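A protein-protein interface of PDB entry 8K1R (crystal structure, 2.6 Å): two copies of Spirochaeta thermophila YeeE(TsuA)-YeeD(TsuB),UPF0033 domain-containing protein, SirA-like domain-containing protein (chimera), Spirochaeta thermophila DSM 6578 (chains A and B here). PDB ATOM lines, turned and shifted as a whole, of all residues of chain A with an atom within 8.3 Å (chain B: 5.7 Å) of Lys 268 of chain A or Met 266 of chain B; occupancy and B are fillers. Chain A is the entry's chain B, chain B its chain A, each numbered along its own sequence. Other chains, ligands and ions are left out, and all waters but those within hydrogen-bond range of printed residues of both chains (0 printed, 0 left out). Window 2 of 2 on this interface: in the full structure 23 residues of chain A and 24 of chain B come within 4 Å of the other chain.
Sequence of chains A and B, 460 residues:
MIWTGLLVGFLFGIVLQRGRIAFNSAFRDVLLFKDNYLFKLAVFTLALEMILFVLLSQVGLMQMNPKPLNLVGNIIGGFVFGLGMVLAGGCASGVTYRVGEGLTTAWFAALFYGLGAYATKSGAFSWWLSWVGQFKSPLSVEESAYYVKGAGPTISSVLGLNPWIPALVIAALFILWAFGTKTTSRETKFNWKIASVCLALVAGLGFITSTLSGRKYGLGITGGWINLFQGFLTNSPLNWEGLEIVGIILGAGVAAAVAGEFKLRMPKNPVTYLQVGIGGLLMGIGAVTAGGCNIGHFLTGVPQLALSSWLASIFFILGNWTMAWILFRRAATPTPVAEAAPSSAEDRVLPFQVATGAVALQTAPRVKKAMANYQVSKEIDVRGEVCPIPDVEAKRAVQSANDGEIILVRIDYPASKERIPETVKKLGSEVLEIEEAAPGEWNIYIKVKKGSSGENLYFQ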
ATOM      1  N   THR A 104      21.332 -15.992 -30.258  1.00  0.00           N
ATOM      2  CA  THR A 104      20.667 -17.250 -30.596  1.00  0.00           C
ATOM      3  C   THR A 104      20.033 -17.911 -29.368  1.00  0.00           C
ATOM      4  O   THR A 104      19.017 -18.607 -29.497  1.00  0.00           O
ATOM      5  CB  THR A 104      21.658 -18.184 -31.289  1.00  0.00           C
ATOM      6  OG1 THR A 104      22.720 -18.529 -30.390  1.00  0.00           O
ATOM      7  CG2 THR A 104      22.260 -17.477 -32.491  1.00  0.00           C
ATOM      8  N   THR A 105      20.576 -17.661 -28.170  1.00  0.00           N
ATOM      9  CA  THR A 105      19.907 -18.118 -26.954  1.00  0.00           C
ATOM     10  C   THR A 105      18.502 -17.534 -26.847  1.00  0.00           C
ATOM     11  O   THR A 105      17.583 -18.192 -26.336  1.00  0.00           O
ATOM     12  CB  THR A 105      20.721 -17.758 -25.698  1.00  0.00           C
ATOM     13  OG1 THR A 105      21.292 -16.450 -25.823  1.00  0.00           O
ATOM     14  CG2 THR A 105      21.824 -18.789 -25.426  1.00  0.00           C
ATOM     15  N   ARG A 265      25.305 -14.177 -31.931  1.00  0.00           N
ATOM     16  CA  ARG A 265      26.004 -14.518 -30.698  1.00  0.00           C
ATOM     17  C   ARG A 265      25.599 -15.900 -30.206  1.00  0.00           C
ATOM     18  O   ARG A 265      24.478 -16.360 -30.439  1.00  0.00           O
ATOM     19  CB  ARG A 265      25.735 -13.496 -29.568  1.00  0.00           C
ATOM     20  CG  ARG A 265      26.478 -12.171 -29.689  1.00  0.00           C
ATOM     21  CD  ARG A 265      25.783 -11.103 -28.840  1.00  0.00           C
ATOM     22  NE  ARG A 265      26.406  -9.789 -28.948  1.00  0.00           N
ATOM     23  CZ  ARG A 265      25.837  -8.742 -29.532  1.00  0.00           C
ATOM     24  NH1 ARG A 265      24.653  -8.841 -30.121  1.00  0.00           N
ATOM     25  NH2 ARG A 265      26.471  -7.568 -29.525  1.00  0.00           N
ATOM     26  N   MET A 266      26.529 -16.538 -29.492  1.00  0.00           N
ATOM     27  CA  MET A 266      26.438 -17.862 -28.896  1.00  0.00           C
ATOM     28  C   MET A 266      26.873 -17.747 -27.444  1.00  0.00           C
ATOM     29  O   MET A 266      27.755 -16.943 -27.125  1.00  0.00           O
ATOM     30  CB  MET A 266      27.373 -18.854 -29.603  1.00  0.00           C
ATOM     31  CG  MET A 266      27.054 -19.131 -31.049  1.00  0.00           C
ATOM     32  SD  MET A 266      27.995 -20.518 -31.750  1.00  0.00           S
ATOM     33  CE  MET A 266      29.681 -19.928 -31.794  1.00  0.00           C
ATOM     34  N   PRO A 267      26.308 -18.544 -26.545  1.00  0.00           N
ATOM     35  CA  PRO A 267      26.766 -18.512 -25.149  1.00  0.00           C
ATOM     36  C   PRO A 267      28.126 -19.183 -25.013  1.00  0.00           C
ATOM     37  O   PRO A 267      28.616 -19.853 -25.922  1.00  0.00           O
ATOM     38  CB  PRO A 267      25.676 -19.285 -24.405  1.00  0.00           C
ATOM     39  CG  PRO A 267      25.171 -20.266 -25.453  1.00  0.00           C
ATOM     40  CD  PRO A 267      25.248 -19.545 -26.766  1.00  0.00           C
ATOM     41  N   LYS A 268      28.741 -19.000 -23.846  1.00  0.00           N
ATOM     42  CA  LYS A 268      30.056 -19.595 -23.610  1.00  0.00           C
ATOM     43  C   LYS A 268      29.988 -21.127 -23.538  1.00  0.00           C
ATOM     44  O   LYS A 268      30.853 -21.821 -24.093  1.00  0.00           O
ATOM     45  CB  LYS A 268      30.667 -19.006 -22.335  1.00  0.00           C
ATOM     46  CG  LYS A 268      32.174 -19.186 -22.237  1.00  0.00           C
ATOM     47  CD  LYS A 268      32.860 -17.889 -21.837  1.00  0.00           C
ATOM     48  CE  LYS A 268      34.373 -18.056 -21.780  1.00  0.00           C
ATOM     49  NZ  LYS A 268      34.796 -19.122 -20.831  1.00  0.00           N
ATOM     50  N   ASN A 269      28.962 -21.678 -22.873  1.00  0.00           N
ATOM     51  CA  ASN A 269      28.809 -23.118 -22.737  1.00  0.00           C
ATOM     52  C   ASN A 269      27.508 -23.582 -23.377  1.00  0.00           C
ATOM     53  O   ASN A 269      26.466 -22.939 -23.202  1.00  0.00           O
ATOM     54  CB  ASN A 269      28.821 -23.544 -21.266  1.00  0.00           C
ATOM     55  CG  ASN A 269      29.942 -22.888 -20.493  1.00  0.00           C
ATOM     56  OD1 ASN A 269      29.735 -21.868 -19.827  1.00  0.00           O
ATOM     57  ND2 ASN A 269      31.155 -23.431 -20.627  1.00  0.00           N
ATOM     58  N   PRO A 270      27.539 -24.693 -24.115  1.00  0.00           N
ATOM     59  CA  PRO A 270      26.327 -25.159 -24.806  1.00  0.00           C
ATOM     60  C   PRO A 270      25.147 -25.442 -23.890  1.00  0.00           C
ATOM     61  O   PRO A 270      24.002 -25.362 -24.350  1.00  0.00           O
ATOM     62  CB  PRO A 270      26.800 -26.434 -25.519  1.00  0.00           C
ATOM     63  CG  PRO A 270      28.264 -26.293 -25.634  1.00  0.00           C
ATOM     64  CD  PRO A 270      28.717 -25.507 -24.443  1.00  0.00           C
ATOM     65  N   VAL A 271      25.374 -25.770 -22.614  1.00  0.00           N
ATOM     66  CA  VAL A 271      24.261 -26.108 -21.733  1.00  0.00           C
ATOM     67  C   VAL A 271      23.306 -24.939 -21.518  1.00  0.00           C
ATOM     68  O   VAL A 271      22.148 -25.154 -21.138  1.00  0.00           O
ATOM     69  CB  VAL A 271      24.803 -26.639 -20.388  1.00  0.00           C
ATOM     70  CG1 VAL A 271      25.449 -25.516 -19.568  1.00  0.00           C
ATOM     71  CG2 VAL A 271      23.692 -27.351 -19.603  1.00  0.00           C
ATOM     72  N   THR A 272      23.757 -23.702 -21.777  1.00  0.00           N
ATOM     73  CA  THR A 272      22.884 -22.535 -21.650  1.00  0.00           C
ATOM     74  C   THR A 272      21.640 -22.665 -22.527  1.00  0.00           C
ATOM     75  O   THR A 272      20.545 -22.224 -22.141  1.00  0.00           O
ATOM     76  CB  THR A 272      23.665 -21.270 -22.005  1.00  0.00           C
ATOM     77  OG1 THR A 272      24.775 -21.136 -21.112  1.00  0.00           O
ATOM     78  CG2 THR A 272      22.784 -20.020 -21.912  1.00  0.00           C
ATOM     79  N   TYR A 273      21.786 -23.271 -23.713  1.00  0.00           N
ATOM     80  CA  TYR A 273      20.632 -23.504 -24.577  1.00  0.00           C
ATOM     81  C   TYR A 273      19.597 -24.375 -23.886  1.00  0.00           C
ATOM     82  O   TYR A 273      18.389 -24.182 -24.070  1.00  0.00           O
ATOM     83  CB  TYR A 273      21.070 -24.148 -25.892  1.00  0.00           C
ATOM     84  CG  TYR A 273      21.792 -23.201 -26.828  1.00  0.00           C
ATOM     85  CD1 TYR A 273      21.110 -22.176 -27.496  1.00  0.00           C
ATOM     86  CD2 TYR A 273      23.154 -23.334 -27.062  1.00  0.00           C
ATOM     87  CE1 TYR A 273      21.775 -21.323 -28.371  1.00  0.00           C
ATOM     88  CE2 TYR A 273      23.826 -22.481 -27.935  1.00  0.00           C
ATOM     89  CZ  TYR A 273      23.139 -21.482 -28.577  1.00  0.00           C
ATOM     90  OH  TYR A 273      23.835 -20.649 -29.425  1.00  0.00           O
ATOM     91  N   ILE A 380      40.543 -11.321 -18.943  1.00  0.00           N
ATOM     92  CA  ILE A 380      39.351 -12.125 -18.711  1.00  0.00           C
ATOM     93  C   ILE A 380      38.454 -12.010 -19.939  1.00  0.00           C
ATOM     94  O   ILE A 380      38.284 -10.919 -20.499  1.00  0.00           O
ATOM     95  CB  ILE A 380      38.614 -11.704 -17.421  1.00  0.00           C
ATOM     96  CG1 ILE A 380      37.845 -10.400 -17.608  1.00  0.00           C
ATOM     97  CG2 ILE A 380      39.599 -11.531 -16.273  1.00  0.00           C
ATOM     98  CD1 ILE A 380      36.723 -10.230 -16.618  1.00  0.00           C
ATOM     99  N   ASP A 381      37.910 -13.143 -20.376  1.00  0.00           N
ATOM    100  CA  ASP A 381      37.088 -13.220 -21.584  1.00  0.00           C
ATOM    101  C   ASP A 381      35.698 -13.688 -21.162  1.00  0.00           C
ATOM    102  O   ASP A 381      35.487 -14.876 -20.892  1.00  0.00           O
ATOM    103  CB  ASP A 381      37.712 -14.165 -22.607  1.00  0.00           C
ATOM    104  CG  ASP A 381      36.993 -14.142 -23.949  1.00  0.00           C
ATOM    105  OD1 ASP A 381      35.957 -13.450 -24.088  1.00  0.00           O
ATOM    106  OD2 ASP A 381      37.470 -14.833 -24.873  1.00  0.00           O
ATOM    107  N   VAL A 382      34.751 -12.756 -21.104  1.00  0.00           N
ATOM    108  CA  VAL A 382      33.388 -13.068 -20.698  1.00  0.00           C
ATOM    109  C   VAL A 382      32.448 -12.872 -21.881  1.00  0.00           C
ATOM    110  O   VAL A 382      31.253 -12.607 -21.703  1.00  0.00           O
ATOM    111  CB  VAL A 382      32.951 -12.223 -19.491  1.00  0.00           C
ATOM    112  CG1 VAL A 382      33.450 -12.854 -18.212  1.00  0.00           C
ATOM    113  CG2 VAL A 382      33.466 -10.797 -19.623  1.00  0.00           C
ATOM    114  N   ARG A 383      32.982 -12.996 -23.092  1.00  0.00           N
ATOM    115  CA  ARG A 383      32.153 -12.954 -24.289  1.00  0.00           C
ATOM    116  C   ARG A 383      31.206 -14.148 -24.293  1.00  0.00           C
ATOM    117  O   ARG A 383      31.642 -15.296 -24.167  1.00  0.00           O
ATOM    118  CB  ARG A 383      33.029 -12.948 -25.536  1.00  0.00           C
ATOM    119  CG  ARG A 383      33.652 -11.592 -25.822  1.00  0.00           C
ATOM    120  CD  ARG A 383      34.519 -11.620 -27.060  1.00  0.00           C
ATOM    121  NE  ARG A 383      35.762 -12.347 -26.837  1.00  0.00           N
ATOM    122  CZ  ARG A 383      36.515 -12.853 -27.804  1.00  0.00           C
ATOM    123  NH1 ARG A 383      36.164 -12.757 -29.076  1.00  0.00           N
ATOM    124  NH2 ARG A 383      37.650 -13.470 -27.488  1.00  0.00           N
ATOM    125  N   GLY A 384      29.909 -13.875 -24.404  1.00  0.00           N
ATOM    126  CA  GLY A 384      28.914 -14.929 -24.403  1.00  0.00           C
ATOM    127  C   GLY A 384      28.495 -15.420 -23.035  1.00  0.00           C
ATOM    128  O   GLY A 384      28.103 -16.586 -22.897  1.00  0.00           O
ATOM    129  N   GLU A 385      28.695 -14.602 -22.012  1.00  0.00           N
ATOM    130  CA  GLU A 385      28.329 -15.034 -20.641  1.00  0.00           C
ATOM    131  C   GLU A 385      27.215 -14.118 -20.153  1.00  0.00           C
ATOM    132  O   GLU A 385      27.133 -12.977 -20.644  1.00  0.00           O
ATOM    133  CB  GLU A 385      29.529 -14.974 -19.698  1.00  0.00           C
ATOM    134  CG  GLU A 385      30.618 -15.967 -20.047  1.00  0.00           C
ATOM    135  CD  GLU A 385      30.946 -16.949 -18.937  1.00  0.00           C
ATOM    136  OE1 GLU A 385      30.131 -17.855 -18.690  1.00  0.00           O
ATOM    137  OE2 GLU A 385      32.017 -16.803 -18.324  1.00  0.00           O
ATOM    138  N   VAL A 386      26.385 -14.620 -19.241  1.00  0.00           N
ATOM    139  CA  VAL A 386      24.999 -14.090 -19.083  1.00  0.00           C
ATOM    140  C   VAL A 386      25.046 -12.809 -18.238  1.00  0.00           C
ATOM    141  O   VAL A 386      25.865 -12.747 -17.324  1.00  0.00           O
ATOM    142  CB  VAL A 386      24.065 -15.163 -18.492  1.00  0.00           C
ATOM    143  CG1 VAL A 386      24.299 -16.523 -19.132  1.00  0.00           C
ATOM    144  CG2 VAL A 386      24.167 -15.256 -16.979  1.00  0.00           C
ATOM    145  N   ILE A 389      27.011 -11.905 -15.391  1.00  0.00           N
ATOM    146  CA  ILE A 389      28.356 -12.533 -15.262  1.00  0.00           C
ATOM    147  C   ILE A 389      29.440 -11.508 -15.616  1.00  0.00           C
ATOM    148  O   ILE A 389      30.351 -11.350 -14.793  1.00  0.00           O
ATOM    149  CB  ILE A 389      28.452 -13.817 -16.111  1.00  0.00           C
ATOM    150  CG1 ILE A 389      27.517 -14.906 -15.582  1.00  0.00           C
ATOM    151  CG2 ILE A 389      29.888 -14.303 -16.202  1.00  0.00           C
ATOM    152  CD1 ILE A 389      28.154 -16.272 -15.490  1.00  0.00           C
ATOM    153  N   ARG A 410      36.936  -8.690 -22.026  1.00  0.00           N
ATOM    154  CA  ARG A 410      36.389  -8.892 -23.361  1.00  0.00           C
ATOM    155  C   ARG A 410      34.905  -9.205 -23.243  1.00  0.00           C
ATOM    156  O   ARG A 410      34.532 -10.223 -22.653  1.00  0.00           O
ATOM    157  CB  ARG A 410      37.123 -10.027 -24.076  1.00  0.00           C
ATOM    158  CG  ARG A 410      38.551  -9.695 -24.454  1.00  0.00           C
ATOM    159  CD  ARG A 410      38.798  -9.971 -25.927  1.00  0.00           C
ATOM    160  NE  ARG A 410      40.142 -10.474 -26.177  1.00  0.00           N
ATOM    161  CZ  ARG A 410      40.831 -10.212 -27.278  1.00  0.00           C
ATOM    162  NH1 ARG A 410      40.326  -9.460 -28.244  1.00  0.00           N
ATOM    163  NH2 ARG A 410      42.059 -10.702 -27.406  1.00  0.00           N
ATOM    164  N   ASP A 412      30.839  -9.093 -25.275  1.00  0.00           N
ATOM    165  CA  ASP A 412      30.060  -8.993 -26.500  1.00  0.00           C
ATOM    166  C   ASP A 412      28.573  -8.828 -26.200  1.00  0.00           C
ATOM    167  O   ASP A 412      27.728  -9.382 -26.911  1.00  0.00           O
ATOM    168  CB  ASP A 412      30.311 -10.199 -27.420  1.00  0.00           C
ATOM    169  CG  ASP A 412      29.772 -11.503 -26.856  1.00  0.00           C
ATOM    170  OD1 ASP A 412      29.573 -11.591 -25.623  1.00  0.00           O
ATOM    171  OD2 ASP A 412      29.546 -12.444 -27.658  1.00  0.00           O
ATOM    172  N   THR B 104      22.948 -28.947 -30.413  1.00  0.00           N
ATOM    173  CA  THR B 104      21.971 -27.866 -30.321  1.00  0.00           C
ATOM    174  C   THR B 104      21.543 -27.371 -31.699  1.00  0.00           C
ATOM    175  O   THR B 104      20.401 -26.924 -31.865  1.00  0.00           O
ATOM    176  CB  THR B 104      22.538 -26.728 -29.486  1.00  0.00           C
ATOM    177  OG1 THR B 104      23.711 -26.202 -30.116  1.00  0.00           O
ATOM    178  CG2 THR B 104      22.924 -27.266 -28.132  1.00  0.00           C
ATOM    179  N   THR B 105      22.418 -27.481 -32.706  1.00  0.00           N
ATOM    180  CA  THR B 105      21.996 -27.195 -34.076  1.00  0.00           C
ATOM    181  C   THR B 105      20.885 -28.133 -34.516  1.00  0.00           C
ATOM    182  O   THR B 105      19.970 -27.729 -35.247  1.00  0.00           O
ATOM    183  CB  THR B 105      23.169 -27.323 -35.043  1.00  0.00           C
ATOM    184  OG1 THR B 105      23.950 -28.464 -34.680  1.00  0.00           O
ATOM    185  CG2 THR B 105      24.033 -26.058 -35.034  1.00  0.00           C
ATOM    186  N   LEU B 264      26.868 -32.030 -25.214  1.00  0.00           N
ATOM    187  CA  LEU B 264      26.174 -30.834 -25.675  1.00  0.00           C
ATOM    188  C   LEU B 264      27.135 -30.014 -26.531  1.00  0.00           C
ATOM    189  O   LEU B 264      28.252 -29.704 -26.106  1.00  0.00           O
ATOM    190  CB  LEU B 264      25.667 -30.026 -24.486  1.00  0.00           C
ATOM    191  CG  LEU B 264      24.600 -30.692 -23.615  1.00  0.00           C
ATOM    192  CD1 LEU B 264      24.066 -29.709 -22.555  1.00  0.00           C
ATOM    193  CD2 LEU B 264      23.453 -31.296 -24.440  1.00  0.00           C
ATOM    194  N   ARG B 265      26.713 -29.701 -27.752  1.00  0.00           N
ATOM    195  CA  ARG B 265      27.594 -29.153 -28.774  1.00  0.00           C
ATOM    196  C   ARG B 265      26.996 -27.887 -29.380  1.00  0.00           C
ATOM    197  O   ARG B 265      25.774 -27.745 -29.502  1.00  0.00           O
ATOM    198  CB  ARG B 265      27.870 -30.176 -29.902  1.00  0.00           C
ATOM    199  CG  ARG B 265      28.839 -31.306 -29.541  1.00  0.00           C
ATOM    200  CD  ARG B 265      28.723 -32.484 -30.544  1.00  0.00           C
ATOM    201  NE  ARG B 265      29.603 -33.602 -30.214  1.00  0.00           N
ATOM    202  CZ  ARG B 265      29.196 -34.805 -29.820  1.00  0.00           C
ATOM    203  NH1 ARG B 265      27.912 -35.082 -29.652  1.00  0.00           N
ATOM    204  NH2 ARG B 265      30.102 -35.755 -29.589  1.00  0.00           N
ATOM    205  N   MET B 266      27.891 -26.971 -29.757  1.00  0.00           N
ATOM    206  CA  MET B 266      27.696 -25.680 -30.392  1.00  0.00           C
ATOM    207  C   MET B 266      28.465 -25.643 -31.709  1.00  0.00           C
ATOM    208  O   MET B 266      29.587 -26.160 -31.782  1.00  0.00           O
ATOM    209  CB  MET B 266      28.215 -24.531 -29.507  1.00  0.00           C
ATOM    210  CG  MET B 266      27.314 -24.108 -28.381  1.00  0.00           C
ATOM    211  SD  MET B 266      27.955 -22.687 -27.438  1.00  0.00           S
ATOM    212  CE  MET B 266      29.669 -23.106 -27.149  1.00  0.00           C
ATOM    213  N   PRO B 267      27.932 -25.004 -32.745  1.00  0.00           N
ATOM    214  CA  PRO B 267      28.701 -24.867 -33.984  1.00  0.00           C
ATOM    215  C   PRO B 267      29.825 -23.860 -33.796  1.00  0.00           C
ATOM    216  O   PRO B 267      29.822 -23.052 -32.865  1.00  0.00           O
ATOM    217  CB  PRO B 267      27.667 -24.362 -34.987  1.00  0.00           C
ATOM    218  CG  PRO B 267      26.739 -23.515 -34.120  1.00  0.00           C
ATOM    219  CD  PRO B 267      26.685 -24.215 -32.776  1.00  0.00           C
ATOM    220  N   LYS B 268      30.788 -23.908 -34.713  1.00  0.00           N
ATOM    221  CA  LYS B 268      31.898 -22.959 -34.680  1.00  0.00           C
ATOM    222  C   LYS B 268      31.420 -21.516 -34.890  1.00  0.00           C
ATOM    223  O   LYS B 268      31.833 -20.608 -34.154  1.00  0.00           O
ATOM    224  CB  LYS B 268      32.934 -23.347 -35.735  1.00  0.00           C
ATOM    225  CG  LYS B 268      34.326 -22.848 -35.438  1.00  0.00           C
ATOM    226  CD  LYS B 268      35.362 -23.887 -35.848  1.00  0.00           C
ATOM    227  CE  LYS B 268      36.633 -23.247 -36.378  1.00  0.00           C
ATOM    228  NZ  LYS B 268      37.038 -22.087 -35.537  1.00  0.00           N
ATOM    229  N   TYR B 273      23.257 -21.534 -37.011  1.00  0.00           N
ATOM    230  CA  TYR B 273      21.896 -21.642 -36.483  1.00  0.00           C
ATOM    231  C   TYR B 273      20.876 -21.088 -37.459  1.00  0.00           C
ATOM    232  O   TYR B 273      19.790 -21.657 -37.623  1.00  0.00           O
ATOM    233  CB  TYR B 273      21.774 -20.920 -35.137  1.00  0.00           C
ATOM    234  CG  TYR B 273      22.407 -21.677 -33.984  1.00  0.00           C
ATOM    235  CD1 TYR B 273      21.887 -22.893 -33.558  1.00  0.00           C
ATOM    236  CD2 TYR B 273      23.535 -21.190 -33.335  1.00  0.00           C
ATOM    237  CE1 TYR B 273      22.461 -23.593 -32.505  1.00  0.00           C
ATOM    238  CE2 TYR B 273      24.116 -21.888 -32.282  1.00  0.00           C
ATOM    239  CZ  TYR B 273      23.575 -23.085 -31.876  1.00  0.00           C
ATOM    240  OH  TYR B 273      24.149 -23.777 -30.838  1.00  0.00           O
ATOM    241  N   ARG B 383      36.506 -28.512 -34.291  1.00  0.00           N
ATOM    242  CA  ARG B 383      35.430 -28.824 -33.366  1.00  0.00           C
ATOM    243  C   ARG B 383      34.234 -27.927 -33.659  1.00  0.00           C
ATOM    244  O   ARG B 383      34.375 -26.707 -33.789  1.00  0.00           O
ATOM    245  CB  ARG B 383      35.913 -28.650 -31.929  1.00  0.00           C
ATOM    246  CG  ARG B 383      36.858 -29.767 -31.479  1.00  0.00           C
ATOM    247  CD  ARG B 383      37.392 -29.547 -30.073  1.00  0.00           C
ATOM    248  NE  ARG B 383      38.052 -28.256 -29.931  1.00  0.00           N
ATOM    249  CZ  ARG B 383      38.676 -27.851 -28.832  1.00  0.00           C
ATOM    250  NH1 ARG B 383      38.741 -28.614 -27.754  1.00  0.00           N
ATOM    251  NH2 ARG B 383      39.238 -26.647 -28.812  1.00  0.00           N
ATOM    252  N   GLY B 384      33.065 -28.542 -33.825  1.00  0.00           N
ATOM    253  CA  GLY B 384      31.846 -27.807 -34.102  1.00  0.00           C
ATOM    254  C   GLY B 384      31.605 -27.428 -35.550  1.00  0.00           C
ATOM    255  O   GLY B 384      30.844 -26.484 -35.806  1.00  0.00           O
ATOM    256  N   ASP B 412      34.953 -33.025 -32.784  1.00  0.00           N
ATOM    257  CA  ASP B 412      33.964 -33.368 -31.771  1.00  0.00           C
ATOM    258  C   ASP B 412      32.683 -33.912 -32.397  1.00  0.00           C
ATOM    259  O   ASP B 412      31.600 -33.730 -31.834  1.00  0.00           O
ATOM    260  CB  ASP B 412      33.658 -32.160 -30.861  1.00  0.00           C
ATOM    261  CG  ASP B 412      32.889 -31.048 -31.567  1.00  0.00           C
ATOM    262  OD1 ASP B 412      32.890 -30.973 -32.821  1.00  0.00           O
ATOM    263  OD2 ASP B 412      32.285 -30.231 -30.839  1.00  0.00           O
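Of the 21 printed residues of chain A, 6 touch a printed residue of chain B.
Hydrophobic or aromatic side chains of chain A that line the printed part of chain B: Met 266, Pro 270, Val 271 and Tyr 273.
Of the 11 printed residues of chain B, 6 touch a printed residue of chain A.
Printed residues of chain B that touch a printed residue of chain A: Leu 264, Arg 265, Met 266, Pro 267, Lys 268 and Tyr 273.
Hydrophobic or aromatic side chains of chain B within 4 Å of the printed part of chain A: Leu 264, Met 266 and Tyr 273.
Among the printed residues, no Asp or Glu carboxylate lies within 4 Å of a Lys or Arg side-chain nitrogen of the other chain.
Met 266 of chain A touches Pro 267 of chain B, and with the chains exchanged Pro 267 of chain A touches Met 266 of chain B.
Met 266 of chain A touches Lys 268 of chain B, and with the chains exchanged Lys 268 of chain A touches Met 266 of chain B.
Tyr 273 of chain A touches Met 266 of chain B, but with the chains exchanged Met 266 of chain A does not touch Tyr 273 of chain B (4.1 Å).
Tyr 273 of chain A touches its own counterpart, Tyr 273 of chain B.
Of the 10 pairs that touch across the chains among the printed residues, 5 have their exchanged pair printed and touching as well.
Printed residues of chain B within 4 Å of Met 266 of chain A: Pro 267 (3.3 Å) and Lys 268 (3.3 Å).
Of the printed residues of chain B, Pro 267 of chain A touches Met 266 (3.3 Å).
Of chain B, only Met 266 comes within 4 Å of Lys 268 of chain A.
Printed residues of chain A within 4 Å of Leu 264 of chain B: Pro 270 and Val 271.
Met 266 of chain B touches just these residues of chain A: Pro 267, Lys 268, Pro 270 and Tyr 273.
The nearest residue of chain A that does not touch Met 266 of chain B is Asn 269 of chain A (4.2 Å).
The side-chain hydroxyl of Tyr 273 of chain A sits close to the side-chain hydroxyl of Tyr 273 of chain B (3.4 Å).
O of Pro 267 of chain B sits close to SD of Met 266 of chain A (3.3 Å).
SD of Met 266 of chain B sits close to O of Pro 267 of chain A (3.3 Å).
The side-chain hydroxyl (OH) of Tyr 273 of chain A lies within hydrogen-bond range of the side-chain hydroxyl (OG1) of Thr 104 of chain A (2.6 Å).
The backbone NH of Lys 268 of chain A sits at hydrogen-bond distance from the backbone carbonyl oxygen of Gly 384 of chain A, 2.7 Å away.
OG1 of Thr 104 of chain B lies within hydrogen-bond range of O of Arg 265 of chain B (2.6 Å).
OG1 of Thr 104 of chain B is in hydrogen-bond range of OH of Tyr 273 of chain B (2.6 Å).
The guanidinium group (NE) of Arg 265 of chain B lies within hydrogen-bond range of the backbone carbonyl oxygen (O) of Asp 412 of chain B (2.6 Å).
N of Lys 268 of chain B sits at hydrogen-bond distance from O of Gly 384 of chain B, at 2.8 Å.
Among the printed residues, merely in contact across the chains: Met 266 of chain A with Lys 268 of chain B, Lys 268 of chain A with Met 266 of chain B, Pro 270 of chain A with Leu 264 of chain B, Pro 270 of chain A with Arg 265 of chain B, Pro 270 of chain A with Met 266 of chain B, Val 271 of chain A with Leu 264 of chain B and Tyr 273 of chain A with Met 266 of chain B.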
